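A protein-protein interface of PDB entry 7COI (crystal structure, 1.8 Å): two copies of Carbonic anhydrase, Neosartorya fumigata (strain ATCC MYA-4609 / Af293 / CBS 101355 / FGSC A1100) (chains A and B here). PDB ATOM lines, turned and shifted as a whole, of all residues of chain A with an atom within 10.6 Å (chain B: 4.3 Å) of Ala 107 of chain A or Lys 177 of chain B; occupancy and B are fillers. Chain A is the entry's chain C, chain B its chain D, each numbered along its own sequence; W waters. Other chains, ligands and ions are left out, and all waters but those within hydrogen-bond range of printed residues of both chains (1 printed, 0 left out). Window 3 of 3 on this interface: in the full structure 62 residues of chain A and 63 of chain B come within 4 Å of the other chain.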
ATOM      1  N   HIS A  99       7.296 -13.998  18.195  1.00  0.00           N
ATOM      2  CA  HIS A  99       7.184 -13.838  16.718  1.00  0.00           C
ATOM      3  C   HIS A  99       5.789 -14.267  16.273  1.00  0.00           C
ATOM      4  O   HIS A  99       5.644 -15.243  15.546  1.00  0.00           O
ATOM      5  CB  HIS A  99       8.297 -14.620  16.000  1.00  0.00           C
ATOM      6  CG  HIS A  99       9.696 -14.250  16.394  1.00  0.00           C
ATOM      7  ND1 HIS A  99      10.287 -13.041  16.022  1.00  0.00           N
ATOM      8  CD2 HIS A  99      10.631 -14.927  17.111  1.00  0.00           C
ATOM      9  CE1 HIS A  99      11.513 -12.987  16.513  1.00  0.00           C
ATOM     10  NE2 HIS A  99      11.747 -14.132  17.196  1.00  0.00           N
ATOM     11  N   PRO A 100       4.717 -13.592  16.739  1.00  0.00           N
ATOM     12  CA  PRO A 100       3.353 -14.118  16.606  1.00  0.00           C
ATOM     13  C   PRO A 100       2.889 -14.282  15.145  1.00  0.00           C
ATOM     14  O   PRO A 100       1.968 -15.012  14.920  1.00  0.00           O
ATOM     15  CB  PRO A 100       2.475 -13.075  17.325  1.00  0.00           C
ATOM     16  CG  PRO A 100       3.327 -11.830  17.387  1.00  0.00           C
ATOM     17  CD  PRO A 100       4.760 -12.294  17.448  1.00  0.00           C
ATOM     18  N   GLU A 101       3.509 -13.574  14.195  1.00  0.00           N
ATOM     19  CA  GLU A 101       3.142 -13.670  12.760  1.00  0.00           C
ATOM     20  C   GLU A 101       3.875 -14.835  12.064  1.00  0.00           C
ATOM     21  O   GLU A 101       3.413 -15.181  10.998  1.00  0.00           O
ATOM     22  CB  GLU A 101       3.372 -12.322  12.067  1.00  0.00           C
ATOM     23  CG  GLU A 101       2.273 -11.322  12.443  1.00  0.00           C
ATOM     24  CD  GLU A 101       2.317  -9.936  11.811  1.00  0.00           C
ATOM     25  OE1 GLU A 101       3.284  -9.625  11.073  1.00  0.00           O
ATOM     26  OE2 GLU A 101       1.363  -9.166  12.060  1.00  0.00           O
ATOM     27  N   LEU A 102       4.954 -15.389  12.614  1.00  0.00           N
ATOM     28  CA  LEU A 102       5.805 -16.385  11.910  1.00  0.00           C
ATOM     29  C   LEU A 102       4.959 -17.605  11.501  1.00  0.00           C
ATOM     30  O   LEU A 102       4.836 -17.856  10.281  1.00  0.00           O
ATOM     31  CB  LEU A 102       6.964 -16.822  12.801  1.00  0.00           C
ATOM     32  CG  LEU A 102       7.894 -17.887  12.205  1.00  0.00           C
ATOM     33  CD1 LEU A 102       8.505 -17.420  10.891  1.00  0.00           C
ATOM     34  CD2 LEU A 102       8.973 -18.271  13.213  1.00  0.00           C
ATOM     35  N   LEU A 103       4.414 -18.359  12.453  1.00  0.00           N
ATOM     36  CA  LEU A 103       3.755 -19.655  12.137  1.00  0.00           C
ATOM     37  C   LEU A 103       2.534 -19.416  11.255  1.00  0.00           C
ATOM     38  O   LEU A 103       2.389 -20.080  10.225  1.00  0.00           O
ATOM     39  CB  LEU A 103       3.470 -20.447  13.416  1.00  0.00           C
ATOM     40  CG  LEU A 103       4.693 -20.840  14.230  1.00  0.00           C
ATOM     41  CD1 LEU A 103       4.279 -21.528  15.539  1.00  0.00           C
ATOM     42  CD2 LEU A 103       5.649 -21.733  13.461  1.00  0.00           C
ATOM     43  N   PRO A 104       1.636 -18.444  11.537  1.00  0.00           N
ATOM     44  CA  PRO A 104       0.513 -18.187  10.634  1.00  0.00           C
ATOM     45  C   PRO A 104       0.965 -17.807   9.212  1.00  0.00           C
ATOM     46  O   PRO A 104       0.301 -18.162   8.287  1.00  0.00           O
ATOM     47  CB  PRO A 104      -0.272 -17.058  11.323  1.00  0.00           C
ATOM     48  CG  PRO A 104       0.126 -17.186  12.787  1.00  0.00           C
ATOM     49  CD  PRO A 104       1.575 -17.622  12.756  1.00  0.00           C
ATOM     50  N   THR A 105       2.063 -17.083   9.042  1.00  0.00           N
ATOM     51  CA  THR A 105       2.540 -16.720   7.676  1.00  0.00           C
ATOM     52  C   THR A 105       3.131 -17.973   7.008  1.00  0.00           C
ATOM     53  O   THR A 105       2.832 -18.201   5.822  1.00  0.00           O
ATOM     54  CB  THR A 105       3.517 -15.546   7.639  1.00  0.00           C
ATOM     55  OG1 THR A 105       4.769 -15.980   8.160  1.00  0.00           O
ATOM     56  CG2 THR A 105       2.976 -14.342   8.377  1.00  0.00           C
ATOM     57  N   LEU A 106       3.861 -18.811   7.746  1.00  0.00           N
ATOM     58  CA  LEU A 106       4.373 -20.098   7.168  1.00  0.00           C
ATOM     59  C   LEU A 106       3.204 -21.005   6.769  1.00  0.00           C
ATOM     60  O   LEU A 106       3.343 -21.715   5.752  1.00  0.00           O
ATOM     61  CB  LEU A 106       5.291 -20.816   8.156  1.00  0.00           C
ATOM     62  CG  LEU A 106       6.615 -20.119   8.436  1.00  0.00           C
ATOM     63  CD1 LEU A 106       7.357 -20.845   9.552  1.00  0.00           C
ATOM     64  CD2 LEU A 106       7.447 -20.089   7.162  1.00  0.00           C
ATOM     65  N   ALA A 107       2.094 -20.991   7.506  1.00  0.00           N
ATOM     66  CA  ALA A 107       0.922 -21.844   7.210  1.00  0.00           C
ATOM     67  C   ALA A 107       0.332 -21.493   5.839  1.00  0.00           C
ATOM     68  O   ALA A 107      -0.378 -22.318   5.279  1.00  0.00           O
ATOM     69  CB  ALA A 107      -0.118 -21.689   8.272  1.00  0.00           C
ATOM     70  N   VAL A 108       0.591 -20.292   5.321  1.00  0.00           N
ATOM     71  CA  VAL A 108       0.034 -19.890   3.992  1.00  0.00           C
ATOM     72  C   VAL A 108       0.779 -20.661   2.901  1.00  0.00           C
ATOM     73  O   VAL A 108       0.179 -20.953   1.881  1.00  0.00           O
ATOM     74  CB  VAL A 108       0.115 -18.372   3.763  1.00  0.00           C
ATOM     75  CG1 VAL A 108      -0.356 -17.984   2.366  1.00  0.00           C
ATOM     76  CG2 VAL A 108      -0.682 -17.627   4.829  1.00  0.00           C
ATOM     77  N   GLY A 109       2.062 -20.947   3.102  1.00  0.00           N
ATOM     78  CA  GLY A 109       2.834 -21.734   2.119  1.00  0.00           C
ATOM     79  C   GLY A 109       4.308 -21.680   2.410  1.00  0.00           C
ATOM     80  O   GLY A 109       4.776 -20.648   2.881  1.00  0.00           O
ATOM     81  N   GLN A 110       5.020 -22.786   2.194  1.00  0.00           N
ATOM     82  CA  GLN A 110       6.479 -22.817   2.448  1.00  0.00           C
ATOM     83  C   GLN A 110       7.225 -22.301   1.208  1.00  0.00           C
ATOM     84  O   GLN A 110       6.761 -22.565   0.114  1.00  0.00           O
ATOM     85  CB  GLN A 110       6.927 -24.226   2.837  1.00  0.00           C
ATOM     86  CG  GLN A 110       6.886 -25.204   1.663  1.00  0.00           C
ATOM     87  CD  GLN A 110       7.359 -26.588   2.039  1.00  0.00           C
ATOM     88  OE1 GLN A 110       8.364 -26.737   2.711  1.00  0.00           O
ATOM     89  NE2 GLN A 110       6.663 -27.598   1.562  1.00  0.00           N
ATOM     90  N   HIS A 111       8.370 -21.677   1.420  1.00  0.00           N
ATOM     91  CA  HIS A 111       9.272 -21.141   0.365  1.00  0.00           C
ATOM     92  C   HIS A 111      10.717 -21.371   0.758  1.00  0.00           C
ATOM     93  O   HIS A 111      11.527 -20.445   0.750  1.00  0.00           O
ATOM     94  CB  HIS A 111       8.961 -19.651   0.129  1.00  0.00           C
ATOM     95  CG  HIS A 111       7.609 -19.468  -0.454  1.00  0.00           C
ATOM     96  ND1 HIS A 111       6.509 -19.176   0.342  1.00  0.00           N
ATOM     97  CD2 HIS A 111       7.150 -19.561  -1.724  1.00  0.00           C
ATOM     98  CE1 HIS A 111       5.430 -19.089  -0.418  1.00  0.00           C
ATOM     99  NE2 HIS A 111       5.793 -19.326  -1.687  1.00  0.00           N
ATOM    100  N   PRO A 134      12.039 -22.668  11.114  1.00  0.00           N
ATOM    101  CA  PRO A 134      11.051 -23.390  10.333  1.00  0.00           C
ATOM    102  C   PRO A 134      10.754 -22.624   9.043  1.00  0.00           C
ATOM    103  O   PRO A 134      10.721 -21.382   9.065  1.00  0.00           O
ATOM    104  CB  PRO A 134       9.819 -23.415  11.252  1.00  0.00           C
ATOM    105  CG  PRO A 134      10.404 -23.313  12.642  1.00  0.00           C
ATOM    106  CD  PRO A 134      11.636 -22.453  12.507  1.00  0.00           C
ATOM    107  N   GLY A 135      10.601 -23.354   7.933  1.00  0.00           N
ATOM    108  CA  GLY A 135      10.358 -22.803   6.589  1.00  0.00           C
ATOM    109  C   GLY A 135      11.625 -22.604   5.780  1.00  0.00           C
ATOM    110  O   GLY A 135      11.498 -22.303   4.618  1.00  0.00           O
ATOM    111  N   PHE A 138      14.072 -27.495   3.435  1.00  0.00           N
ATOM    112  CA  PHE A 138      13.373 -28.739   3.003  1.00  0.00           C
ATOM    113  C   PHE A 138      14.339 -29.895   3.215  1.00  0.00           C
ATOM    114  O   PHE A 138      15.505 -29.782   2.805  1.00  0.00           O
ATOM    115  CB  PHE A 138      12.882 -28.600   1.579  1.00  0.00           C
ATOM    116  CG  PHE A 138      11.850 -29.611   1.183  1.00  0.00           C
ATOM    117  CD1 PHE A 138      10.543 -29.495   1.608  1.00  0.00           C
ATOM    118  CD2 PHE A 138      12.153 -30.634   0.304  1.00  0.00           C
ATOM    119  CE1 PHE A 138       9.571 -30.385   1.203  1.00  0.00           C
ATOM    120  CE2 PHE A 138      11.172 -31.532  -0.104  1.00  0.00           C
ATOM    121  CZ  PHE A 138       9.898 -31.436   0.379  1.00  0.00           C
ATOM    122  N   PHE A 160      10.404 -33.027  -5.745  1.00  0.00           N
ATOM    123  CA  PHE A 160       9.503 -32.044  -5.091  1.00  0.00           C
ATOM    124  C   PHE A 160      10.258 -30.746  -4.805  1.00  0.00           C
ATOM    125  O   PHE A 160       9.746 -29.652  -5.173  1.00  0.00           O
ATOM    126  CB  PHE A 160       8.871 -32.637  -3.831  1.00  0.00           C
ATOM    127  CG  PHE A 160       7.693 -31.832  -3.352  1.00  0.00           C
ATOM    128  CD1 PHE A 160       7.883 -30.737  -2.526  1.00  0.00           C
ATOM    129  CD2 PHE A 160       6.410 -32.126  -3.789  1.00  0.00           C
ATOM    130  CE1 PHE A 160       6.799 -29.979  -2.103  1.00  0.00           C
ATOM    131  CE2 PHE A 160       5.327 -31.356  -3.382  1.00  0.00           C
ATOM    132  CZ  PHE A 160       5.525 -30.289  -2.537  1.00  0.00           C
ATOM    133  N   LEU A 165       9.115 -26.725  -5.363  1.00  0.00           N
ATOM    134  CA  LEU A 165       9.485 -25.609  -4.451  1.00  0.00           C
ATOM    135  C   LEU A 165      10.553 -24.712  -5.097  1.00  0.00           C
ATOM    136  O   LEU A 165      10.764 -23.605  -4.609  1.00  0.00           O
ATOM    137  CB  LEU A 165       9.960 -26.180  -3.113  1.00  0.00           C
ATOM    138  CG  LEU A 165       8.926 -27.006  -2.355  1.00  0.00           C
ATOM    139  CD1 LEU A 165       9.520 -27.505  -1.041  1.00  0.00           C
ATOM    140  CD2 LEU A 165       7.660 -26.196  -2.104  1.00  0.00           C
ATOM    141  N   ASP B 121       8.787 -31.428   4.597  1.00  0.00           N
ATOM    142  CA  ASP B 121       8.222 -30.053   4.679  1.00  0.00           C
ATOM    143  C   ASP B 121       9.128 -29.189   5.559  1.00  0.00           C
ATOM    144  O   ASP B 121       9.424 -29.578   6.722  1.00  0.00           O
ATOM    145  CB  ASP B 121       6.777 -30.080   5.161  1.00  0.00           C
ATOM    146  CG  ASP B 121       6.059 -28.744   5.006  1.00  0.00           C
ATOM    147  OD1 ASP B 121       6.540 -27.760   5.590  1.00  0.00           O
ATOM    148  OD2 ASP B 121       5.068 -28.705   4.295  1.00  0.00           O
ATOM    149  N   ARG B 123       8.658 -26.683   7.210  1.00  0.00           N
ATOM    150  CA  ARG B 123       7.997 -26.133   8.421  1.00  0.00           C
ATOM    151  C   ARG B 123       7.975 -27.163   9.554  1.00  0.00           C
ATOM    152  O   ARG B 123       7.463 -26.795  10.645  1.00  0.00           O
ATOM    153  CB  ARG B 123       6.586 -25.653   8.088  1.00  0.00           C
ATOM    154  CG  ARG B 123       6.604 -24.600   6.987  1.00  0.00           C
ATOM    155  CD  ARG B 123       5.264 -24.355   6.382  1.00  0.00           C
ATOM    156  NE  ARG B 123       4.752 -25.498   5.658  1.00  0.00           N
ATOM    157  CZ  ARG B 123       3.595 -25.524   5.007  1.00  0.00           C
ATOM    158  NH1 ARG B 123       2.790 -24.468   4.993  1.00  0.00           N
ATOM    159  NH2 ARG B 123       3.257 -26.599   4.334  1.00  0.00           N
ATOM    160  N   HIS B 175       1.437 -33.752   9.220  1.00  0.00           N
ATOM    161  CA  HIS B 175       1.240 -32.300   9.488  1.00  0.00           C
ATOM    162  C   HIS B 175       0.128 -31.770   8.614  1.00  0.00           C
ATOM    163  O   HIS B 175      -0.265 -32.395   7.620  1.00  0.00           O
ATOM    164  CB  HIS B 175       2.578 -31.524   9.368  1.00  0.00           C
ATOM    165  CG  HIS B 175       3.002 -31.468   7.941  1.00  0.00           C
ATOM    166  ND1 HIS B 175       2.828 -30.314   7.158  1.00  0.00           N
ATOM    167  CD2 HIS B 175       3.522 -32.418   7.135  1.00  0.00           C
ATOM    168  CE1 HIS B 175       3.243 -30.568   5.924  1.00  0.00           C
ATOM    169  NE2 HIS B 175       3.657 -31.803   5.944  1.00  0.00           N
ATOM    170  N   THR B 176      -0.429 -30.637   9.036  1.00  0.00           N
ATOM    171  CA  THR B 176      -1.465 -29.921   8.280  1.00  0.00           C
ATOM    172  C   THR B 176      -0.776 -29.253   7.084  1.00  0.00           C
ATOM    173  O   THR B 176       0.435 -28.912   7.169  1.00  0.00           O
ATOM    174  CB  THR B 176      -2.201 -28.939   9.214  1.00  0.00           C
ATOM    175  OG1 THR B 176      -1.257 -27.949   9.635  1.00  0.00           O
ATOM    176  CG2 THR B 176      -2.803 -29.627  10.417  1.00  0.00           C
ATOM    177  N   LYS B 177      -1.529 -29.025   6.020  1.00  0.00           N
ATOM    178  CA  LYS B 177      -1.059 -28.335   4.794  1.00  0.00           C
ATOM    179  C   LYS B 177       0.058 -29.165   4.143  1.00  0.00           C
ATOM    180  O   LYS B 177       1.036 -28.556   3.646  1.00  0.00           O
ATOM    181  CB  LYS B 177      -0.579 -26.926   5.117  1.00  0.00           C
ATOM    182  CG  LYS B 177      -1.548 -26.102   5.963  1.00  0.00           C
ATOM    183  CD  LYS B 177      -2.858 -25.814   5.344  1.00  0.00           C
ATOM    184  CE  LYS B 177      -2.711 -24.722   4.310  1.00  0.00           C
ATOM    185  NZ  LYS B 177      -3.977 -24.534   3.565  1.00  0.00           N
ATOM    186  N   CYS B 178      -0.035 -30.496   4.207  1.00  0.00           N
ATOM    187  CA  CYS B 178       0.982 -31.404   3.605  1.00  0.00           C
ATOM    188  C   CYS B 178       0.783 -31.443   2.089  1.00  0.00           C
ATOM    189  O   CYS B 178      -0.248 -31.941   1.663  1.00  0.00           O
ATOM    190  CB  CYS B 178       0.933 -32.806   4.212  1.00  0.00           C
ATOM    191  SG  CYS B 178       2.288 -33.852   3.577  1.00  0.00           S
ATOM    192  N   GLY B 179       1.803 -31.010   1.342  1.00  0.00           N
ATOM    193  CA  GLY B 179       1.844 -31.032  -0.132  1.00  0.00           C
ATOM    194  C   GLY B 179       1.733 -32.441  -0.710  1.00  0.00           C
ATOM    195  O   GLY B 179       1.132 -32.608  -1.775  1.00  0.00           O
ATOM    196  N   ASP B 217      -9.965 -28.773   2.513  1.00  0.00           N
ATOM    197  CA  ASP B 217      -9.012 -28.540   3.621  1.00  0.00           C
ATOM    198  C   ASP B 217      -9.205 -29.631   4.673  1.00  0.00           C
ATOM    199  O   ASP B 217      -8.184 -30.093   5.215  1.00  0.00           O
ATOM    200  CB  ASP B 217      -9.133 -27.113   4.160  1.00  0.00           C
ATOM    201  CG  ASP B 217      -8.490 -26.110   3.217  1.00  0.00           C
ATOM    202  OD1 ASP B 217      -7.403 -26.440   2.680  1.00  0.00           O
ATOM    203  OD2 ASP B 217      -9.076 -25.011   3.026  1.00  0.00           O
ATOM    204  N   VAL B 259       1.014 -26.600  11.398  1.00  0.00           N
ATOM    205  CA  VAL B 259       2.076 -25.660  10.953  1.00  0.00           C
ATOM    206  C   VAL B 259       1.674 -24.215  11.303  1.00  0.00           C
ATOM    207  O   VAL B 259       2.570 -23.376  11.329  1.00  0.00           O
ATOM    208  CB  VAL B 259       2.384 -25.814   9.449  1.00  0.00           C
ATOM    209  CG1 VAL B 259       2.875 -27.218   9.132  1.00  0.00           C
ATOM    210  CG2 VAL B 259       1.183 -25.486   8.581  1.00  0.00           C
ATOM    211  N   GLY B 260       0.384 -23.955  11.520  1.00  0.00           N
ATOM    212  CA  GLY B 260      -0.148 -22.606  11.814  1.00  0.00           C
ATOM    213  C   GLY B 260      -0.066 -22.219  13.287  1.00  0.00           C
ATOM    214  O   GLY B 260      -0.077 -21.020  13.561  1.00  0.00           O
HETATM  215  O   HOH W   1       0.802 -24.506   3.005  1.00  0.00           O
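NH1 of Arg 123 of chain B is in hydrogen-bond range of O of Leu 106 of chain A (2.9 Å). The side-chain amide nitrogen (NE2) of Gln 110 of chain A sits at hydrogen-bond distance from the side-chain carboxylate (OD2) of Asp 121 of chain B. O of Leu 103 of chain A lies close to O of Val 259 of chain B, at 3.5 Å.
The backbone carbonyl oxygen (O) of Gly 109 of chain A sits at hydrogen-bond distance from a ring nitrogen (ND1) of His 111 of chain A, 3.4 Å away. The side-chain carboxylate (OD2) of Asp 121 of chain B is in salt-bridge range of the guanidinium group (NH2) of Arg 123 of chain B, 2.8 Å away. The guanidinium group (NH2) of Arg 123 of chain B is in hydrogen-bond range of the backbone carbonyl oxygen (O) of Lys 177 of chain B. The side-chain hydroxyl (OG1) of Thr 176 of chain B sits at hydrogen-bond distance from the backbone NH (N) of Val 259 of chain B.
Among the printed residues, merely in contact across the chains: Ala 107 of chain A with Lys 177 of chain B (3.5 Å), Leu 103 of chain A with Gly 260 of chain B (3.6 Å), Phe 138 of chain A with Asp 121 of chain B (3.6 Å), Ala 107 of chain A with Gly 260 of chain B (3.7 Å), Pro 104 of chain A with Gly 260 of chain B (3.7 Å), Gln 110 of chain A with Arg 123 of chain B (3.8 Å), Ala 107 of chain A with Arg 123 of chain B (3.8 Å), Gly 135 of chain A with Arg 123 of chain B (3.8 Å), Ala 107 of chain A with Val 259 of chain B (3.9 Å) and Gly 109 of chain A with Arg 123 of chain B (3.97 Å).
Of chain B, only Arg 123 (3.8 Å), Lys 177 (3.5 Å), Val 259 (3.9 Å) and Gly 260 (3.7 Å) come within 4 Å of Ala 107 of chain A. Lys 177 of chain B touches just one residue of chain A: Ala 107. No residue of chain A comes within 4 Å of His 175 of chain B. No residue of chain A comes within 4 Å of Thr 176 of chain B. No residue of chain A comes within 4 Å of Cys 178 of chain B. Of chain A, only Leu 103 and Ala 107 come within 4 Å of Val 259 of chain B. Gly 260 of chain B touches just these residues of chain A: Leu 103 (3.6 Å), Pro 104 (3.7 Å) and Ala 107 (3.7 Å). Of the printed residues of chain B, Gly 109 of chain A touches Arg 123 (3.97 Å). Printed residues of chain B within 4 Å of Phe 138 of chain A: Asp 121 (3.6 Å). Of the printed residues of chain B, Pro 104 of chain A touches Gly 260 (3.7 Å). Of the printed residues of chain A, Asp 121 of chain B touches Gln 110 (3.4 Å) and Phe 138 (3.6 Å). Phe 160 of chain A touches none of the printed residues of chain B. The nearest printed residue of chain B that does not touch Ala 107 of chain A is Thr 176 of chain B (6.5 Å).
Hydrophobic or aromatic side chains of chain B within 4 Å of the printed part of chain A: Val 259. Among the printed residues, 13 pairs touch across the chains. Among the printed residues, no Asp or Glu carboxylate lies within 4 Å of a Lys or Arg side-chain nitrogen of the other chain.
No position is printed for both chains. Of the 13 pairs that touch across the chains among the printed residues, none has its exchanged pair printed and touching as well.
Water W1 lies within hydrogen-bond range of NH1 of Arg 123 of chain B (2.8 Å) and O of Ala 107 of chain A (3.4 Å).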
